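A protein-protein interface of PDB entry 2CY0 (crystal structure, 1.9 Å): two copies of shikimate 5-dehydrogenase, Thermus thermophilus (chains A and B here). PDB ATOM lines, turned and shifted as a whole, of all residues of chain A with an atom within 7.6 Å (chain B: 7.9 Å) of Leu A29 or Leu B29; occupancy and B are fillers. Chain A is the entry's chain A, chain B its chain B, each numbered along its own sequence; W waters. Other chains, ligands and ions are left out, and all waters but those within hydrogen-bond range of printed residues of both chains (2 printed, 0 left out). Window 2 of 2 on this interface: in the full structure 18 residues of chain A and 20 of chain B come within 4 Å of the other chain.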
ATOM      1  N   MET A   1     -27.627   7.974  30.485  1.00  0.00           N
ATOM      2  CA  MET A   1     -26.317   8.525  30.815  1.00  0.00           C
ATOM      3  C   MET A   1     -25.997   9.747  29.952  1.00  0.00           C
ATOM      4  O   MET A   1     -26.660  10.042  28.968  1.00  0.00           O
ATOM      5  CB  MET A   1     -25.272   7.424  30.621  1.00  0.00           C
ATOM      6  CG  MET A   1     -25.542   6.212  31.512  1.00  0.00           C
ATOM      7  SD  MET A   1     -24.606   4.762  31.007  1.00  0.00           S
ATOM      8  CE  MET A   1     -25.810   4.059  29.868  1.00  0.00           C
ATOM      9  N   LEU A   2     -24.960  10.490  30.383  1.00  0.00           N
ATOM     10  CA  LEU A   2     -24.547  11.666  29.630  1.00  0.00           C
ATOM     11  C   LEU A   2     -25.587  12.789  29.664  1.00  0.00           C
ATOM     12  O   LEU A   2     -26.331  13.035  28.719  1.00  0.00           O
ATOM     13  CB  LEU A   2     -24.272  11.225  28.193  1.00  0.00           C
ATOM     14  CG  LEU A   2     -22.978  10.407  28.096  1.00  0.00           C
ATOM     15  CD1 LEU A   2     -22.380  10.383  26.689  1.00  0.00           C
ATOM     16  CD2 LEU A   2     -21.882  10.935  29.022  1.00  0.00           C
ATOM     17  N   PHE A   4     -25.833  16.725  29.857  1.00  0.00           N
ATOM     18  CA  PHE A   4     -25.021  17.923  29.740  1.00  0.00           C
ATOM     19  C   PHE A   4     -25.907  19.159  29.739  1.00  0.00           C
ATOM     20  O   PHE A   4     -27.134  19.068  29.697  1.00  0.00           O
ATOM     21  CB  PHE A   4     -24.194  17.907  28.448  1.00  0.00           C
ATOM     22  CG  PHE A   4     -23.249  16.762  28.339  1.00  0.00           C
ATOM     23  CD1 PHE A   4     -23.394  15.845  27.315  1.00  0.00           C
ATOM     24  CD2 PHE A   4     -22.193  16.614  29.236  1.00  0.00           C
ATOM     25  CE1 PHE A   4     -22.502  14.784  27.176  1.00  0.00           C
ATOM     26  CE2 PHE A   4     -21.294  15.554  29.106  1.00  0.00           C
ATOM     27  CZ  PHE A   4     -21.448  14.639  28.075  1.00  0.00           C
ATOM     28  N   HIS A  20     -24.621  19.996  20.371  1.00  0.00           N
ATOM     29  CA  HIS A  20     -24.380  18.785  21.145  1.00  0.00           C
ATOM     30  C   HIS A  20     -25.385  17.667  20.897  1.00  0.00           C
ATOM     31  O   HIS A  20     -25.061  16.479  21.042  1.00  0.00           O
ATOM     32  CB  HIS A  20     -24.278  19.149  22.624  1.00  0.00           C
ATOM     33  CG  HIS A  20     -23.049  19.948  22.946  1.00  0.00           C
ATOM     34  ND1 HIS A  20     -21.819  19.366  23.153  1.00  0.00           N
ATOM     35  CD2 HIS A  20     -22.848  21.288  23.003  1.00  0.00           C
ATOM     36  CE1 HIS A  20     -20.909  20.314  23.323  1.00  0.00           C
ATOM     37  NE2 HIS A  20     -21.506  21.486  23.235  1.00  0.00           N
ATOM     38  N   ALA A  21     -26.602  18.040  20.516  1.00  0.00           N
ATOM     39  CA  ALA A  21     -27.608  17.040  20.202  1.00  0.00           C
ATOM     40  C   ALA A  21     -27.001  16.298  19.016  1.00  0.00           C
ATOM     41  O   ALA A  21     -27.015  15.068  18.969  1.00  0.00           O
ATOM     42  CB  ALA A  21     -28.937  17.714  19.807  1.00  0.00           C
ATOM     43  N   ALA A  23     -23.791  16.089  18.213  1.00  0.00           N
ATOM     44  CA  ALA A  23     -22.606  15.354  18.644  1.00  0.00           C
ATOM     45  C   ALA A  23     -23.005  13.972  19.159  1.00  0.00           C
ATOM     46  O   ALA A  23     -22.446  12.957  18.743  1.00  0.00           O
ATOM     47  CB  ALA A  23     -21.881  16.126  19.748  1.00  0.00           C
ATOM     48  N   LEU A  24     -23.961  13.943  20.082  1.00  0.00           N
ATOM     49  CA  LEU A  24     -24.429  12.682  20.651  1.00  0.00           C
ATOM     50  C   LEU A  24     -24.932  11.743  19.549  1.00  0.00           C
ATOM     51  O   LEU A  24     -24.487  10.598  19.438  1.00  0.00           O
ATOM     52  CB  LEU A  24     -25.540  12.965  21.666  1.00  0.00           C
ATOM     53  CG  LEU A  24     -25.089  13.697  22.938  1.00  0.00           C
ATOM     54  CD1 LEU A  24     -26.290  14.254  23.671  1.00  0.00           C
ATOM     55  CD2 LEU A  24     -24.305  12.746  23.833  1.00  0.00           C
ATOM     56  N   GLU A  25     -25.847  12.245  18.727  1.00  0.00           N
ATOM     57  CA  GLU A  25     -26.420  11.473  17.630  1.00  0.00           C
ATOM     58  C   GLU A  25     -25.316  10.932  16.726  1.00  0.00           C
ATOM     59  O   GLU A  25     -25.236   9.732  16.485  1.00  0.00           O
ATOM     60  CB  GLU A  25     -27.369  12.364  16.812  1.00  0.00           C
ATOM     61  CG  GLU A  25     -28.181  11.663  15.718  1.00  0.00           C
ATOM     62  CD  GLU A  25     -27.338  10.815  14.771  1.00  0.00           C
ATOM     63  OE1 GLU A  25     -27.135   9.615  15.066  1.00  0.00           O
ATOM     64  OE2 GLU A  25     -26.873  11.345  13.737  1.00  0.00           O
ATOM     65  N   SER A  26     -24.464  11.826  16.234  1.00  0.00           N
ATOM     66  CA  SER A  26     -23.378  11.449  15.332  1.00  0.00           C
ATOM     67  C   SER A  26     -22.459  10.360  15.882  1.00  0.00           C
ATOM     68  O   SER A  26     -21.880   9.587  15.120  1.00  0.00           O
ATOM     69  CB  SER A  26     -22.533  12.678  14.986  1.00  0.00           C
ATOM     70  OG  SER A  26     -21.760  13.087  16.101  1.00  0.00           O
ATOM     71  N   LEU A  27     -22.311  10.310  17.198  1.00  0.00           N
ATOM     72  CA  LEU A  27     -21.438   9.320  17.810  1.00  0.00           C
ATOM     73  C   LEU A  27     -22.215   8.101  18.308  1.00  0.00           C
ATOM     74  O   LEU A  27     -21.649   7.211  18.938  1.00  0.00           O
ATOM     75  CB  LEU A  27     -20.663   9.965  18.961  1.00  0.00           C
ATOM     76  CG  LEU A  27     -19.774  11.147  18.557  1.00  0.00           C
ATOM     77  CD1 LEU A  27     -19.301  11.872  19.802  1.00  0.00           C
ATOM     78  CD2 LEU A  27     -18.593  10.658  17.735  1.00  0.00           C
ATOM     79  N   GLY A  28     -23.514   8.069  18.027  1.00  0.00           N
ATOM     80  CA  GLY A  28     -24.327   6.941  18.448  1.00  0.00           C
ATOM     81  C   GLY A  28     -24.446   6.814  19.952  1.00  0.00           C
ATOM     82  O   GLY A  28     -24.517   5.709  20.498  1.00  0.00           O
ATOM     83  N   LEU A  29     -24.479   7.953  20.630  1.00  0.00           N
ATOM     84  CA  LEU A  29     -24.590   7.969  22.084  1.00  0.00           C
ATOM     85  C   LEU A  29     -25.959   8.491  22.507  1.00  0.00           C
ATOM     86  O   LEU A  29     -26.566   9.295  21.806  1.00  0.00           O
ATOM     87  CB  LEU A  29     -23.506   8.870  22.684  1.00  0.00           C
ATOM     88  CG  LEU A  29     -22.041   8.521  22.421  1.00  0.00           C
ATOM     89  CD1 LEU A  29     -21.157   9.672  22.876  1.00  0.00           C
ATOM     90  CD2 LEU A  29     -21.677   7.243  23.156  1.00  0.00           C
ATOM     91  N   GLU A  30     -26.446   8.024  23.651  1.00  0.00           N
ATOM     92  CA  GLU A  30     -27.731   8.483  24.169  1.00  0.00           C
ATOM     93  C   GLU A  30     -27.433   9.548  25.207  1.00  0.00           C
ATOM     94  O   GLU A  30     -26.499   9.407  25.992  1.00  0.00           O
ATOM     95  CB  GLU A  30     -28.497   7.334  24.825  1.00  0.00           C
ATOM     96  CG  GLU A  30     -29.140   6.361  23.851  1.00  0.00           C
ATOM     97  CD  GLU A  30     -30.251   6.999  23.037  1.00  0.00           C
ATOM     98  OE1 GLU A  30     -31.169   7.592  23.643  1.00  0.00           O
ATOM     99  OE2 GLU A  30     -30.209   6.902  21.792  1.00  0.00           O
ATOM    100  N   GLY A  31     -28.216  10.616  25.213  1.00  0.00           N
ATOM    101  CA  GLY A  31     -27.981  11.668  26.180  1.00  0.00           C
ATOM    102  C   GLY A  31     -28.710  12.950  25.840  1.00  0.00           C
ATOM    103  O   GLY A  31     -29.470  13.003  24.877  1.00  0.00           O
ATOM    104  N   SER A  32     -28.471  13.987  26.628  1.00  0.00           N
ATOM    105  CA  SER A  32     -29.126  15.259  26.400  1.00  0.00           C
ATOM    106  C   SER A  32     -28.242  16.433  26.786  1.00  0.00           C
ATOM    107  O   SER A  32     -27.374  16.320  27.647  1.00  0.00           O
ATOM    108  CB  SER A  32     -30.423  15.323  27.208  1.00  0.00           C
ATOM    109  OG  SER A  32     -30.156  15.200  28.597  1.00  0.00           O
ATOM    110  N   PHE A 240     -16.755  18.407  24.396  1.00  0.00           N
ATOM    111  CA  PHE A 240     -17.348  17.073  24.340  1.00  0.00           C
ATOM    112  C   PHE A 240     -16.281  15.997  24.553  1.00  0.00           C
ATOM    113  O   PHE A 240     -16.532  14.981  25.206  1.00  0.00           O
ATOM    114  CB  PHE A 240     -18.043  16.842  22.994  1.00  0.00           C
ATOM    115  CG  PHE A 240     -19.066  15.727  23.021  1.00  0.00           C
ATOM    116  CD1 PHE A 240     -20.380  15.976  23.411  1.00  0.00           C
ATOM    117  CD2 PHE A 240     -18.709  14.429  22.680  1.00  0.00           C
ATOM    118  CE1 PHE A 240     -21.319  14.950  23.467  1.00  0.00           C
ATOM    119  CE2 PHE A 240     -19.642  13.395  22.732  1.00  0.00           C
ATOM    120  CZ  PHE A 240     -20.948  13.656  23.125  1.00  0.00           C
ATOM    121  N   THR A 244     -16.204  12.990  27.304  1.00  0.00           N
ATOM    122  CA  THR A 244     -16.331  11.588  26.916  1.00  0.00           C
ATOM    123  C   THR A 244     -15.111  10.884  26.357  1.00  0.00           C
ATOM    124  O   THR A 244     -15.057   9.653  26.365  1.00  0.00           O
ATOM    125  CB  THR A 244     -17.427  11.417  25.855  1.00  0.00           C
ATOM    126  OG1 THR A 244     -16.993  12.030  24.630  1.00  0.00           O
ATOM    127  CG2 THR A 244     -18.737  12.066  26.323  1.00  0.00           C
ATOM    128  N   LEU A 246     -14.333  11.354  23.287  1.00  0.00           N
ATOM    129  CA  LEU A 246     -14.651  11.288  21.857  1.00  0.00           C
ATOM    130  C   LEU A 246     -14.732  12.695  21.267  1.00  0.00           C
ATOM    131  O   LEU A 246     -15.257  13.610  21.903  1.00  0.00           O
ATOM    132  CB  LEU A 246     -15.985  10.568  21.651  1.00  0.00           C
ATOM    133  CG  LEU A 246     -16.047   9.131  22.186  1.00  0.00           C
ATOM    134  CD1 LEU A 246     -17.496   8.692  22.311  1.00  0.00           C
ATOM    135  CD2 LEU A 246     -15.276   8.206  21.267  1.00  0.00           C
ATOM    136  N   MET B   1     -10.295   6.797  18.593  1.00  0.00           N
ATOM    137  CA  MET B   1     -10.504   5.454  19.204  1.00  0.00           C
ATOM    138  C   MET B   1     -10.235   5.624  20.704  1.00  0.00           C
ATOM    139  O   MET B   1      -9.386   6.435  21.076  1.00  0.00           O
ATOM    140  CB  MET B   1      -9.529   4.441  18.611  1.00  0.00           C
ATOM    141  CG  MET B   1      -9.914   3.029  19.049  1.00  0.00           C
ATOM    142  SD  MET B   1      -9.919   1.791  17.707  1.00  0.00           S
ATOM    143  CE  MET B   1      -9.181   0.370  18.391  1.00  0.00           C
ATOM    144  N   LEU B   2     -10.984   4.938  21.572  1.00  0.00           N
ATOM    145  CA  LEU B   2     -10.756   5.072  23.022  1.00  0.00           C
ATOM    146  C   LEU B   2      -9.626   4.130  23.398  1.00  0.00           C
ATOM    147  O   LEU B   2      -9.676   2.946  23.073  1.00  0.00           O
ATOM    148  CB  LEU B   2     -12.024   4.730  23.825  1.00  0.00           C
ATOM    149  CG  LEU B   2     -13.173   5.747  23.765  1.00  0.00           C
ATOM    150  CD1 LEU B   2     -14.400   5.226  24.509  1.00  0.00           C
ATOM    151  CD2 LEU B   2     -12.713   7.066  24.371  1.00  0.00           C
ATOM    152  N   PHE B   4      -7.439   2.412  26.437  1.00  0.00           N
ATOM    153  CA  PHE B   4      -7.353   2.111  27.865  1.00  0.00           C
ATOM    154  C   PHE B   4      -6.330   1.016  28.119  1.00  0.00           C
ATOM    155  O   PHE B   4      -5.927   0.301  27.196  1.00  0.00           O
ATOM    156  CB  PHE B   4      -8.705   1.640  28.397  1.00  0.00           C
ATOM    157  CG  PHE B   4      -9.810   2.627  28.226  1.00  0.00           C
ATOM    158  CD1 PHE B   4     -10.879   2.349  27.383  1.00  0.00           C
ATOM    159  CD2 PHE B   4      -9.784   3.840  28.905  1.00  0.00           C
ATOM    160  CE1 PHE B   4     -11.919   3.258  27.232  1.00  0.00           C
ATOM    161  CE2 PHE B   4     -10.819   4.759  28.764  1.00  0.00           C
ATOM    162  CZ  PHE B   4     -11.886   4.468  27.920  1.00  0.00           C
ATOM    163  N   HIS B  20     -13.441  -4.900  30.285  1.00  0.00           N
ATOM    164  CA  HIS B  20     -13.577  -3.664  29.546  1.00  0.00           C
ATOM    165  C   HIS B  20     -13.819  -3.896  28.062  1.00  0.00           C
ATOM    166  O   HIS B  20     -14.351  -3.024  27.379  1.00  0.00           O
ATOM    167  CB  HIS B  20     -12.354  -2.788  29.819  1.00  0.00           C
ATOM    168  CG  HIS B  20     -12.309  -2.263  31.226  1.00  0.00           C
ATOM    169  ND1 HIS B  20     -12.979  -1.129  31.614  1.00  0.00           N
ATOM    170  CD2 HIS B  20     -11.699  -2.744  32.337  1.00  0.00           C
ATOM    171  CE1 HIS B  20     -12.784  -0.925  32.909  1.00  0.00           C
ATOM    172  NE2 HIS B  20     -12.014  -1.890  33.369  1.00  0.00           N
ATOM    173  N   ALA B  21     -13.442  -5.072  27.565  1.00  0.00           N
ATOM    174  CA  ALA B  21     -13.691  -5.407  26.170  1.00  0.00           C
ATOM    175  C   ALA B  21     -15.208  -5.528  26.063  1.00  0.00           C
ATOM    176  O   ALA B  21     -15.807  -5.130  25.064  1.00  0.00           O
ATOM    177  CB  ALA B  21     -13.029  -6.727  25.804  1.00  0.00           C
ATOM    178  N   PHE B  22     -15.823  -6.081  27.106  1.00  0.00           N
ATOM    179  CA  PHE B  22     -17.277  -6.219  27.143  1.00  0.00           C
ATOM    180  C   PHE B  22     -17.909  -4.843  27.286  1.00  0.00           C
ATOM    181  O   PHE B  22     -18.935  -4.558  26.670  1.00  0.00           O
ATOM    182  CB  PHE B  22     -17.726  -7.109  28.309  1.00  0.00           C
ATOM    183  CG  PHE B  22     -19.153  -6.893  28.715  1.00  0.00           C
ATOM    184  CD1 PHE B  22     -19.462  -6.075  29.795  1.00  0.00           C
ATOM    185  CD2 PHE B  22     -20.192  -7.463  27.990  1.00  0.00           C
ATOM    186  CE1 PHE B  22     -20.783  -5.830  30.148  1.00  0.00           C
ATOM    187  CE2 PHE B  22     -21.518  -7.225  28.333  1.00  0.00           C
ATOM    188  CZ  PHE B  22     -21.816  -6.403  29.413  1.00  0.00           C
ATOM    189  N   ALA B  23     -17.303  -3.991  28.105  1.00  0.00           N
ATOM    190  CA  ALA B  23     -17.822  -2.644  28.302  1.00  0.00           C
ATOM    191  C   ALA B  23     -17.883  -1.929  26.954  1.00  0.00           C
ATOM    192  O   ALA B  23     -18.937  -1.435  26.553  1.00  0.00           O
ATOM    193  CB  ALA B  23     -16.930  -1.865  29.266  1.00  0.00           C
ATOM    194  N   LEU B  24     -16.747  -1.889  26.263  1.00  0.00           N
ATOM    195  CA  LEU B  24     -16.643  -1.235  24.962  1.00  0.00           C
ATOM    196  C   LEU B  24     -17.681  -1.749  23.969  1.00  0.00           C
ATOM    197  O   LEU B  24     -18.439  -0.965  23.391  1.00  0.00           O
ATOM    198  CB  LEU B  24     -15.235  -1.437  24.385  1.00  0.00           C
ATOM    199  CG  LEU B  24     -14.108  -0.621  25.027  1.00  0.00           C
ATOM    200  CD1 LEU B  24     -12.749  -1.140  24.583  1.00  0.00           C
ATOM    201  CD2 LEU B  24     -14.275   0.838  24.642  1.00  0.00           C
ATOM    202  N   GLU B  25     -17.712  -3.064  23.780  1.00  0.00           N
ATOM    203  CA  GLU B  25     -18.645  -3.697  22.851  1.00  0.00           C
ATOM    204  C   GLU B  25     -20.114  -3.482  23.207  1.00  0.00           C
ATOM    205  O   GLU B  25     -20.907  -3.068  22.362  1.00  0.00           O
ATOM    206  CB  GLU B  25     -18.360  -5.197  22.775  1.00  0.00           C
ATOM    207  CG  GLU B  25     -19.279  -5.957  21.841  1.00  0.00           C
ATOM    208  CD  GLU B  25     -19.095  -7.455  21.959  1.00  0.00           C
ATOM    209  OE1 GLU B  25     -19.264  -7.983  23.079  1.00  0.00           O
ATOM    210  OE2 GLU B  25     -18.781  -8.105  20.937  1.00  0.00           O
ATOM    211  N   SER B  26     -20.479  -3.772  24.451  1.00  0.00           N
ATOM    212  CA  SER B  26     -21.862  -3.615  24.885  1.00  0.00           C
ATOM    213  C   SER B  26     -22.340  -2.172  24.806  1.00  0.00           C
ATOM    214  O   SER B  26     -23.535  -1.919  24.656  1.00  0.00           O
ATOM    215  CB  SER B  26     -22.041  -4.129  26.320  1.00  0.00           C
ATOM    216  OG  SER B  26     -21.275  -3.370  27.237  1.00  0.00           O
ATOM    217  N   LEU B  27     -21.417  -1.223  24.910  1.00  0.00           N
ATOM    218  CA  LEU B  27     -21.794   0.183  24.850  1.00  0.00           C
ATOM    219  C   LEU B  27     -21.644   0.756  23.445  1.00  0.00           C
ATOM    220  O   LEU B  27     -21.772   1.965  23.240  1.00  0.00           O
ATOM    221  CB  LEU B  27     -20.953   0.993  25.834  1.00  0.00           C
ATOM    222  CG  LEU B  27     -21.185   0.684  27.315  1.00  0.00           C
ATOM    223  CD1 LEU B  27     -20.109   1.350  28.151  1.00  0.00           C
ATOM    224  CD2 LEU B  27     -22.568   1.165  27.737  1.00  0.00           C
ATOM    225  N   GLY B  28     -21.378  -0.117  22.477  1.00  0.00           N
ATOM    226  CA  GLY B  28     -21.219   0.328  21.104  1.00  0.00           C
ATOM    227  C   GLY B  28     -20.115   1.349  20.908  1.00  0.00           C
ATOM    228  O   GLY B  28     -20.236   2.250  20.080  1.00  0.00           O
ATOM    229  N   LEU B  29     -19.028   1.215  21.660  1.00  0.00           N
ATOM    230  CA  LEU B  29     -17.914   2.148  21.537  1.00  0.00           C
ATOM    231  C   LEU B  29     -16.709   1.474  20.899  1.00  0.00           C
ATOM    232  O   LEU B  29     -16.493   0.274  21.073  1.00  0.00           O
ATOM    233  CB  LEU B  29     -17.528   2.691  22.915  1.00  0.00           C
ATOM    234  CG  LEU B  29     -18.567   3.567  23.617  1.00  0.00           C
ATOM    235  CD1 LEU B  29     -18.144   3.802  25.063  1.00  0.00           C
ATOM    236  CD2 LEU B  29     -18.703   4.890  22.873  1.00  0.00           C
ATOM    237  N   GLU B  30     -15.930   2.246  20.154  1.00  0.00           N
ATOM    238  CA  GLU B  30     -14.736   1.720  19.511  1.00  0.00           C
ATOM    239  C   GLU B  30     -13.510   2.048  20.346  1.00  0.00           C
ATOM    240  O   GLU B  30     -13.297   3.193  20.731  1.00  0.00           O
ATOM    241  CB  GLU B  30     -14.575   2.311  18.109  1.00  0.00           C
ATOM    242  CG  GLU B  30     -15.521   1.721  17.086  1.00  0.00           C
ATOM    243  CD  GLU B  30     -15.300   0.232  16.895  1.00  0.00           C
ATOM    244  OE1 GLU B  30     -14.189  -0.150  16.468  1.00  0.00           O
ATOM    245  OE2 GLU B  30     -16.231  -0.556  17.175  1.00  0.00           O
ATOM    246  N   GLY B  31     -12.698   1.035  20.621  1.00  0.00           N
ATOM    247  CA  GLY B  31     -11.505   1.263  21.409  1.00  0.00           C
ATOM    248  C   GLY B  31     -10.909  -0.031  21.904  1.00  0.00           C
ATOM    249  O   GLY B  31     -11.328  -1.116  21.494  1.00  0.00           O
ATOM    250  N   SER B  32      -9.933   0.077  22.797  1.00  0.00           N
ATOM    251  CA  SER B  32      -9.296  -1.111  23.324  1.00  0.00           C
ATOM    252  C   SER B  32      -8.795  -0.931  24.749  1.00  0.00           C
ATOM    253  O   SER B  32      -8.568   0.183  25.208  1.00  0.00           O
ATOM    254  CB  SER B  32      -8.134  -1.518  22.419  1.00  0.00           C
ATOM    255  OG  SER B  32      -7.212  -0.454  22.284  1.00  0.00           O
ATOM    256  N   PHE B 240     -14.797   2.809  34.169  1.00  0.00           N
ATOM    257  CA  PHE B 240     -15.229   3.103  32.807  1.00  0.00           C
ATOM    258  C   PHE B 240     -16.126   4.343  32.777  1.00  0.00           C
ATOM    259  O   PHE B 240     -15.977   5.195  31.900  1.00  0.00           O
ATOM    260  CB  PHE B 240     -15.978   1.908  32.205  1.00  0.00           C
ATOM    261  CG  PHE B 240     -15.999   1.901  30.702  1.00  0.00           C
ATOM    262  CD1 PHE B 240     -14.959   1.318  29.984  1.00  0.00           C
ATOM    263  CD2 PHE B 240     -17.006   2.551  30.006  1.00  0.00           C
ATOM    264  CE1 PHE B 240     -14.934   1.363  28.592  1.00  0.00           C
ATOM    265  CE2 PHE B 240     -16.994   2.605  28.609  1.00  0.00           C
ATOM    266  CZ  PHE B 240     -15.951   2.020  27.902  1.00  0.00           C
ATOM    267  N   THR B 244     -15.491   7.712  30.567  1.00  0.00           N
ATOM    268  CA  THR B 244     -16.406   8.091  29.499  1.00  0.00           C
ATOM    269  C   THR B 244     -17.738   8.718  29.894  1.00  0.00           C
ATOM    270  O   THR B 244     -18.357   9.424  29.097  1.00  0.00           O
ATOM    271  CB  THR B 244     -16.734   6.869  28.636  1.00  0.00           C
ATOM    272  OG1 THR B 244     -17.568   5.976  29.384  1.00  0.00           O
ATOM    273  CG2 THR B 244     -15.458   6.129  28.243  1.00  0.00           C
ATOM    274  N   GLY B 245     -18.186   8.448  31.113  1.00  0.00           N
ATOM    275  CA  GLY B 245     -19.465   8.967  31.542  1.00  0.00           C
ATOM    276  C   GLY B 245     -20.548   7.913  31.361  1.00  0.00           C
ATOM    277  O   GLY B 245     -21.701   8.125  31.740  1.00  0.00           O
ATOM    278  N   LEU B 246     -20.183   6.776  30.775  1.00  0.00           N
ATOM    279  CA  LEU B 246     -21.133   5.690  30.558  1.00  0.00           C
ATOM    280  C   LEU B 246     -20.803   4.524  31.487  1.00  0.00           C
ATOM    281  O   LEU B 246     -19.643   4.123  31.601  1.00  0.00           O
ATOM    282  CB  LEU B 246     -21.085   5.200  29.108  1.00  0.00           C
ATOM    283  CG  LEU B 246     -21.492   6.138  27.971  1.00  0.00           C
ATOM    284  CD1 LEU B 246     -20.505   7.285  27.867  1.00  0.00           C
ATOM    285  CD2 LEU B 246     -21.515   5.362  26.669  1.00  0.00           C
HETATM  286  O   HOH W   1     -23.677   3.754  23.071  1.00  0.00           O
HETATM  287  O   HOH W   2     -22.384  10.257  32.709  1.00  0.00           O
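Among the printed residues, pairs that only touch across the chains: Met A1 with Leu B246, Thr A244 with Thr B244, Leu A29 with Leu B29, Met A1 with Gly B245, Leu A2 with Leu B246, Leu A2 with Thr B244, Leu A2 with Gly B245 and Leu A29 with Leu B246.
Gly A28 touches none of the printed residues of chain B.
Printed residues of chain B within 4 Å of Leu A29: Leu B29 and Leu B246.
Phe B4 touches none of the printed residues of chain A.
Ala B23 touches none of the printed residues of chain A.
No residue of chain A comes within 4 Å of Gly B28.
Of chain A, only Leu A29 (3.8 Å) comes within 4 Å of Leu B29.
Of the printed residues of chain A, Gly B245 touches Met A1 (3.8 Å) and Leu A2 (3.9 Å).
Of the printed residues of chain A, Leu B246 touches Met A1, Leu A2 and Leu A29.
The nearest printed residue of chain B that does not touch Leu A29 is Leu B27 (5.3 Å).
The nearest residue of chain A that does not touch Leu B29 is Leu A246 (4.03 Å).
The nearest printed residue of chain A that does not touch Thr B244 is Phe A4 (6.1 Å).
Met A1 touches Leu B246, but with the chains exchanged Leu A246 does not touch Met B1 (5.7 Å).
Leu A2 touches Thr B244, but with the chains exchanged Thr A244 does not touch Leu B2 (4.02 Å).
Leu A2 touches Leu B246, but with the chains exchanged Leu A246 does not touch Leu B2 (4.1 Å).
Leu A29 touches Leu B246, but with the chains exchanged Leu A246 does not touch Leu B29 (4.03 Å).
18 positions are printed for both chains.
Of the 8 pairs that touch across the chains among the printed residues, 2 have their exchanged pair printed and touching as well.
The backbone carbonyl oxygen (O) of Leu A2 is in hydrogen-bond range of the backbone NH (N) of Ser A32 (3.1 Å).
The backbone carbonyl oxygen of Leu B24 sits at hydrogen-bond distance from the backbone NH of Leu B29, at 2.8 Å.
N of Leu B246 lies within hydrogen-bond range of OG1 of Thr B244 (3.1 Å).
The side-chain hydroxyl (OG1) of Thr B244 lies within hydrogen-bond range of the backbone carbonyl oxygen (O) of Phe B240 (3.1 Å).
The backbone NH (N) of Leu A246 is in hydrogen-bond range of the side-chain hydroxyl (OG1) of Thr A244 (3.1 Å).
OG1 of Thr A244 sits at hydrogen-bond distance from O of Phe A240, at 3.0 Å.
Water W2 lies within hydrogen-bond range of the backbone carbonyl oxygen (O) of Gly B245 (2.4 Å) and the backbone NH (N) of Leu A2 (3.5 Å).
Water W1 lies within hydrogen-bond range of O of Leu B27 (2.6 Å) and O of Gly A28 (3.3 Å).
Printed residues of chain A that touch a printed residue of chain B: Met A1, Leu A2, Leu A29 and Thr A244.
Hydrophobic or aromatic side chains of chain A that line the printed part of chain B: Met A1, Leu A2 and Leu A29.
Of the 20 printed residues of chain B, 4 touch a printed residue of chain A.
Printed residues of chain B that touch a printed residue of chain A: Leu B29, Thr B244, Gly B245 and Leu B246.
Hydrophobic or aromatic side chains of chain B that line the printed part of chain A: Leu B29 and Leu B246.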
